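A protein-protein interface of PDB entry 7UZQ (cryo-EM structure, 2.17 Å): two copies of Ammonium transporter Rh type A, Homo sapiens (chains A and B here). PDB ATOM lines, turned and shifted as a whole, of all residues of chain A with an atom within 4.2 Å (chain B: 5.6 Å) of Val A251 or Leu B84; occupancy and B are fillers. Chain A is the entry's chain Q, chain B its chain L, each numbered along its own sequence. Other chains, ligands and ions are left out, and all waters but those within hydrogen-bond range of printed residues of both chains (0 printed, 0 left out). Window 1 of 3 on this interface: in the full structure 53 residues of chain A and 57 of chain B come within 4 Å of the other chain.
The indole nitrogen of Trp A219 sits at hydrogen-bond distance from the backbone carbonyl oxygen of Leu A247, at 3.5 Å. NE1 of Trp A219 lies close to O of Thr A276, at 3.3 Å.
Among the printed residues, pairs that only touch across the chains: Phe A255 with Gly B81, Trp A219 with Phe B62, Leu A216 with Phe B62, Val A251 with Ala B88, Leu A216 with Val B80, Leu A252 with Leu B89, Ala A248 with Ala B88, Val A251 with Leu B85, Phe A255 with Leu B85, Val A251 with Leu B84 and Leu A252 with Leu B85.
Of the printed residues of chain B, Trp A219 touches Phe B62 (3.3 Å). Of the printed residues of chain B, Ala A248 touches Ala B88 (3.8 Å). Cys A250 touches none of the printed residues of chain B. Of chain B, only Leu B84 (3.9 Å), Leu B85 (3.8 Å) and Ala B88 (3.6 Å) come within 4 Å of Val A251. Thr A276 touches none of the printed residues of chain B. Of the printed residues of chain A, Phe B62 touches Leu A216 (3.4 Å) and Trp A219 (3.3 Å). Of the printed residues of chain A, Gly B81 touches Phe A255. Of chain A, only Val A251 comes within 4 Å of Leu B84. Of the printed residues of chain A, Leu B85 touches Val A251, Leu A252 and Phe A255. The nearest printed residue of chain B that does not touch Val A251 is Leu B89 (5.8 Å).
Hydrophobic or aromatic side chains of chain B within 4 Å of the printed part of chain A: Phe B62, Val B80, Leu B84, Leu B85 and Ala B88. Printed residues of chain A that touch a printed residue of chain B: Leu A216, Trp A219, Ala A248, Val A251, Leu A252 and Phe A255. Hydrophobic or aromatic side chains of chain A that line the printed part of chain B: Leu A216, Trp A219, Ala A248, Val A251, Leu A252 and Phe A255. Among the printed residues, no Asp or Glu carboxylate lies within 4 Å of a Lys or Arg side-chain nitrogen of the other chain.
No position is printed for both chains. Of the 11 pairs that touch across the chains among the printed residues, none has its exchanged pair printed and touching as well.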
ATOM      1  N   LEU A 216      24.065   2.185  24.262  1.00  0.00           N
ATOM      2  CA  LEU A 216      23.234   1.053  24.635  1.00  0.00           C
ATOM      3  C   LEU A 216      23.954   0.139  25.609  1.00  0.00           C
ATOM      4  O   LEU A 216      23.329  -0.408  26.519  1.00  0.00           O
ATOM      5  CB  LEU A 216      22.784   0.286  23.390  1.00  0.00           C
ATOM      6  CG  LEU A 216      21.701   0.983  22.558  1.00  0.00           C
ATOM      7  CD1 LEU A 216      21.385   0.182  21.316  1.00  0.00           C
ATOM      8  CD2 LEU A 216      20.438   1.224  23.371  1.00  0.00           C
ATOM      9  N   TRP A 219      23.685   1.825  28.936  1.00  0.00           N
ATOM     10  CA  TRP A 219      22.309   1.765  29.409  1.00  0.00           C
ATOM     11  C   TRP A 219      21.961   0.379  29.934  1.00  0.00           C
ATOM     12  O   TRP A 219      21.314   0.245  30.977  1.00  0.00           O
ATOM     13  CB  TRP A 219      21.377   2.155  28.266  1.00  0.00           C
ATOM     14  CG  TRP A 219      20.000   2.487  28.677  1.00  0.00           C
ATOM     15  CD1 TRP A 219      19.529   3.707  29.042  1.00  0.00           C
ATOM     16  CD2 TRP A 219      18.892   1.591  28.747  1.00  0.00           C
ATOM     17  NE1 TRP A 219      18.200   3.630  29.345  1.00  0.00           N
ATOM     18  CE2 TRP A 219      17.780   2.340  29.173  1.00  0.00           C
ATOM     19  CE3 TRP A 219      18.731   0.226  28.494  1.00  0.00           C
ATOM     20  CZ2 TRP A 219      16.527   1.775  29.353  1.00  0.00           C
ATOM     21  CZ3 TRP A 219      17.491  -0.334  28.674  1.00  0.00           C
ATOM     22  CH2 TRP A 219      16.399   0.438  29.094  1.00  0.00           C
ATOM     23  N   LEU A 247      16.317   4.031  34.547  1.00  0.00           N
ATOM     24  CA  LEU A 247      16.772   4.193  33.169  1.00  0.00           C
ATOM     25  C   LEU A 247      15.609   4.074  32.189  1.00  0.00           C
ATOM     26  O   LEU A 247      15.529   4.836  31.211  1.00  0.00           O
ATOM     27  CB  LEU A 247      17.853   3.160  32.854  1.00  0.00           C
ATOM     28  CG  LEU A 247      19.247   3.460  33.403  1.00  0.00           C
ATOM     29  CD1 LEU A 247      20.088   2.205  33.387  1.00  0.00           C
ATOM     30  CD2 LEU A 247      19.930   4.567  32.614  1.00  0.00           C
ATOM     31  N   ALA A 248      14.693   3.130  32.438  1.00  0.00           N
ATOM     32  CA  ALA A 248      13.518   3.015  31.575  1.00  0.00           C
ATOM     33  C   ALA A 248      12.735   4.327  31.522  1.00  0.00           C
ATOM     34  O   ALA A 248      12.397   4.814  30.439  1.00  0.00           O
ATOM     35  CB  ALA A 248      12.619   1.874  32.049  1.00  0.00           C
ATOM     36  N   ALA A 249      12.438   4.916  32.684  1.00  0.00           N
ATOM     37  CA  ALA A 249      11.668   6.162  32.705  1.00  0.00           C
ATOM     38  C   ALA A 249      12.441   7.307  32.054  1.00  0.00           C
ATOM     39  O   ALA A 249      11.860   8.167  31.362  1.00  0.00           O
ATOM     40  CB  ALA A 249      11.298   6.520  34.142  1.00  0.00           C
ATOM     41  N   CYS A 250      13.753   7.336  32.283  1.00  0.00           N
ATOM     42  CA  CYS A 250      14.591   8.377  31.719  1.00  0.00           C
ATOM     43  C   CYS A 250      14.549   8.357  30.199  1.00  0.00           C
ATOM     44  O   CYS A 250      14.611   9.412  29.564  1.00  0.00           O
ATOM     45  CB  CYS A 250      16.023   8.207  32.220  1.00  0.00           C
ATOM     46  SG  CYS A 250      17.167   9.415  31.597  1.00  0.00           S
ATOM     47  N   VAL A 251      14.458   7.169  29.592  1.00  0.00           N
ATOM     48  CA  VAL A 251      14.380   7.110  28.131  1.00  0.00           C
ATOM     49  C   VAL A 251      13.157   7.874  27.634  1.00  0.00           C
ATOM     50  O   VAL A 251      13.238   8.672  26.690  1.00  0.00           O
ATOM     51  CB  VAL A 251      14.363   5.650  27.639  1.00  0.00           C
ATOM     52  CG1 VAL A 251      13.879   5.576  26.184  1.00  0.00           C
ATOM     53  CG2 VAL A 251      15.734   5.033  27.772  1.00  0.00           C
ATOM     54  N   LEU A 252      12.001   7.633  28.257  1.00  0.00           N
ATOM     55  CA  LEU A 252      10.770   8.275  27.813  1.00  0.00           C
ATOM     56  C   LEU A 252      10.877   9.786  27.932  1.00  0.00           C
ATOM     57  O   LEU A 252      10.554  10.521  26.989  1.00  0.00           O
ATOM     58  CB  LEU A 252       9.579   7.760  28.626  1.00  0.00           C
ATOM     59  CG  LEU A 252       8.878   6.495  28.127  1.00  0.00           C
ATOM     60  CD1 LEU A 252       8.020   6.800  26.912  1.00  0.00           C
ATOM     61  CD2 LEU A 252       9.886   5.394  27.823  1.00  0.00           C
ATOM     62  N   THR A 253      11.362  10.271  29.077  1.00  0.00           N
ATOM     63  CA  THR A 253      11.426  11.723  29.239  1.00  0.00           C
ATOM     64  C   THR A 253      12.483  12.343  28.329  1.00  0.00           C
ATOM     65  O   THR A 253      12.293  13.449  27.813  1.00  0.00           O
ATOM     66  CB  THR A 253      11.685  12.105  30.697  1.00  0.00           C
ATOM     67  OG1 THR A 253      12.878  11.470  31.168  1.00  0.00           O
ATOM     68  CG2 THR A 253      10.505  11.697  31.565  1.00  0.00           C
ATOM     69  N   ALA A 254      13.605  11.653  28.119  1.00  0.00           N
ATOM     70  CA  ALA A 254      14.655  12.192  27.265  1.00  0.00           C
ATOM     71  C   ALA A 254      14.176  12.314  25.824  1.00  0.00           C
ATOM     72  O   ALA A 254      14.380  13.347  25.180  1.00  0.00           O
ATOM     73  CB  ALA A 254      15.908  11.320  27.355  1.00  0.00           C
ATOM     74  N   PHE A 255      13.505  11.280  25.310  1.00  0.00           N
ATOM     75  CA  PHE A 255      12.916  11.376  23.975  1.00  0.00           C
ATOM     76  C   PHE A 255      11.907  12.516  23.904  1.00  0.00           C
ATOM     77  O   PHE A 255      11.920  13.322  22.963  1.00  0.00           O
ATOM     78  CB  PHE A 255      12.243  10.056  23.598  1.00  0.00           C
ATOM     79  CG  PHE A 255      13.134   9.109  22.859  1.00  0.00           C
ATOM     80  CD1 PHE A 255      13.997   8.271  23.544  1.00  0.00           C
ATOM     81  CD2 PHE A 255      13.107   9.048  21.478  1.00  0.00           C
ATOM     82  CE1 PHE A 255      14.818   7.397  22.863  1.00  0.00           C
ATOM     83  CE2 PHE A 255      13.926   8.177  20.799  1.00  0.00           C
ATOM     84  CZ  PHE A 255      14.780   7.350  21.491  1.00  0.00           C
ATOM     85  N   THR A 276      19.600   9.752  27.752  1.00  0.00           N
ATOM     86  CA  THR A 276      18.939   8.501  28.109  1.00  0.00           C
ATOM     87  C   THR A 276      19.652   7.751  29.235  1.00  0.00           C
ATOM     88  O   THR A 276      19.087   6.795  29.770  1.00  0.00           O
ATOM     89  CB  THR A 276      18.822   7.598  26.878  1.00  0.00           C
ATOM     90  OG1 THR A 276      20.117   7.395  26.304  1.00  0.00           O
ATOM     91  CG2 THR A 276      17.898   8.215  25.841  1.00  0.00           C
ATOM     92  N   PHE B  62      18.051  -4.927  23.381  1.00  0.00           N
ATOM     93  CA  PHE B  62      18.375  -3.547  23.042  1.00  0.00           C
ATOM     94  C   PHE B  62      19.460  -3.430  21.977  1.00  0.00           C
ATOM     95  O   PHE B  62      19.401  -2.520  21.147  1.00  0.00           O
ATOM     96  CB  PHE B  62      18.762  -2.787  24.307  1.00  0.00           C
ATOM     97  CG  PHE B  62      17.588  -2.477  25.178  1.00  0.00           C
ATOM     98  CD1 PHE B  62      16.869  -1.309  25.005  1.00  0.00           C
ATOM     99  CD2 PHE B  62      17.179  -3.375  26.146  1.00  0.00           C
ATOM    100  CE1 PHE B  62      15.774  -1.037  25.798  1.00  0.00           C
ATOM    101  CE2 PHE B  62      16.087  -3.109  26.935  1.00  0.00           C
ATOM    102  CZ  PHE B  62      15.380  -1.942  26.759  1.00  0.00           C
ATOM    103  N   SER B  79      15.646   3.131  13.539  1.00  0.00           N
ATOM    104  CA  SER B  79      15.652   1.729  13.939  1.00  0.00           C
ATOM    105  C   SER B  79      16.216   1.570  15.351  1.00  0.00           C
ATOM    106  O   SER B  79      15.504   1.142  16.265  1.00  0.00           O
ATOM    107  CB  SER B  79      16.420   0.889  12.910  1.00  0.00           C
ATOM    108  OG  SER B  79      17.765   0.694  13.273  1.00  0.00           O
ATOM    109  N   VAL B  80      17.463   1.993  15.575  1.00  0.00           N
ATOM    110  CA  VAL B  80      18.070   1.749  16.886  1.00  0.00           C
ATOM    111  C   VAL B  80      17.386   2.579  17.982  1.00  0.00           C
ATOM    112  O   VAL B  80      17.082   2.065  19.068  1.00  0.00           O
ATOM    113  CB  VAL B  80      19.595   1.983  16.822  1.00  0.00           C
ATOM    114  CG1 VAL B  80      19.943   3.451  16.702  1.00  0.00           C
ATOM    115  CG2 VAL B  80      20.281   1.368  18.037  1.00  0.00           C
ATOM    116  N   GLY B  81      17.106   3.859  17.720  1.00  0.00           N
ATOM    117  CA  GLY B  81      16.542   4.715  18.751  1.00  0.00           C
ATOM    118  C   GLY B  81      15.106   4.380  19.108  1.00  0.00           C
ATOM    119  O   GLY B  81      14.744   4.360  20.287  1.00  0.00           O
ATOM    120  N   ILE B  82      14.257   4.140  18.106  1.00  0.00           N
ATOM    121  CA  ILE B  82      12.886   3.752  18.396  1.00  0.00           C
ATOM    122  C   ILE B  82      12.856   2.361  19.004  1.00  0.00           C
ATOM    123  O   ILE B  82      11.975   2.064  19.809  1.00  0.00           O
ATOM    124  CB  ILE B  82      12.013   3.849  17.130  1.00  0.00           C
ATOM    125  CG1 ILE B  82      12.074   5.264  16.521  1.00  0.00           C
ATOM    126  CG2 ILE B  82      10.581   3.451  17.432  1.00  0.00           C
ATOM    127  CD1 ILE B  82      11.749   6.401  17.472  1.00  0.00           C
ATOM    128  N   ASN B  83      13.813   1.492  18.661  1.00  0.00           N
ATOM    129  CA  ASN B  83      13.953   0.247  19.404  1.00  0.00           C
ATOM    130  C   ASN B  83      14.151   0.533  20.887  1.00  0.00           C
ATOM    131  O   ASN B  83      13.449  -0.027  21.737  1.00  0.00           O
ATOM    132  CB  ASN B  83      15.121  -0.565  18.840  1.00  0.00           C
ATOM    133  CG  ASN B  83      15.137  -1.997  19.332  1.00  0.00           C
ATOM    134  OD1 ASN B  83      14.492  -2.868  18.751  1.00  0.00           O
ATOM    135  ND2 ASN B  83      15.886  -2.250  20.393  1.00  0.00           N
ATOM    136  N   LEU B  84      15.085   1.431  21.211  1.00  0.00           N
ATOM    137  CA  LEU B  84      15.337   1.768  22.611  1.00  0.00           C
ATOM    138  C   LEU B  84      14.081   2.327  23.277  1.00  0.00           C
ATOM    139  O   LEU B  84      13.716   1.915  24.380  1.00  0.00           O
ATOM    140  CB  LEU B  84      16.497   2.763  22.711  1.00  0.00           C
ATOM    141  CG  LEU B  84      16.747   3.480  24.048  1.00  0.00           C
ATOM    142  CD1 LEU B  84      17.071   2.489  25.167  1.00  0.00           C
ATOM    143  CD2 LEU B  84      17.866   4.493  23.907  1.00  0.00           C
ATOM    144  N   LEU B  85      13.401   3.253  22.604  1.00  0.00           N
ATOM    145  CA  LEU B  85      12.226   3.900  23.184  1.00  0.00           C
ATOM    146  C   LEU B  85      11.092   2.901  23.400  1.00  0.00           C
ATOM    147  O   LEU B  85      10.494   2.838  24.484  1.00  0.00           O
ATOM    148  CB  LEU B  85      11.776   5.041  22.273  1.00  0.00           C
ATOM    149  CG  LEU B  85      10.382   5.653  22.449  1.00  0.00           C
ATOM    150  CD1 LEU B  85      10.283   6.374  23.779  1.00  0.00           C
ATOM    151  CD2 LEU B  85      10.079   6.592  21.300  1.00  0.00           C
ATOM    152  N   VAL B  86      10.778   2.122  22.365  1.00  0.00           N
ATOM    153  CA  VAL B  86       9.710   1.137  22.444  1.00  0.00           C
ATOM    154  C   VAL B  86       9.999   0.140  23.550  1.00  0.00           C
ATOM    155  O   VAL B  86       9.114  -0.195  24.335  1.00  0.00           O
ATOM    156  CB  VAL B  86       9.536   0.438  21.081  1.00  0.00           C
ATOM    157  CG1 VAL B  86       8.846  -0.910  21.228  1.00  0.00           C
ATOM    158  CG2 VAL B  86       8.761   1.321  20.127  1.00  0.00           C
ATOM    159  N   ALA B  87      11.237  -0.349  23.634  1.00  0.00           N
ATOM    160  CA  ALA B  87      11.554  -1.354  24.637  1.00  0.00           C
ATOM    161  C   ALA B  87      11.541  -0.764  26.043  1.00  0.00           C
ATOM    162  O   ALA B  87      11.122  -1.432  26.992  1.00  0.00           O
ATOM    163  CB  ALA B  87      12.903  -1.994  24.322  1.00  0.00           C
ATOM    164  N   ALA B  88      11.984   0.486  26.201  1.00  0.00           N
ATOM    165  CA  ALA B  88      11.937   1.126  27.512  1.00  0.00           C
ATOM    166  C   ALA B  88      10.500   1.279  27.993  1.00  0.00           C
ATOM    167  O   ALA B  88      10.192   1.005  29.157  1.00  0.00           O
ATOM    168  CB  ALA B  88      12.635   2.484  27.465  1.00  0.00           C
ATOM    169  N   LEU B  89       9.603   1.727  27.112  1.00  0.00           N
ATOM    170  CA  LEU B  89       8.193   1.791  27.490  1.00  0.00           C
ATOM    171  C   LEU B  89       7.635   0.397  27.741  1.00  0.00           C
ATOM    172  O   LEU B  89       6.872   0.178  28.694  1.00  0.00           O
ATOM    173  CB  LEU B  89       7.386   2.497  26.399  1.00  0.00           C
ATOM    174  CG  LEU B  89       5.860   2.476  26.549  1.00  0.00           C
ATOM    175  CD1 LEU B  89       5.441   3.130  27.860  1.00  0.00           C
ATOM    176  CD2 LEU B  89       5.187   3.154  25.371  1.00  0.00           C
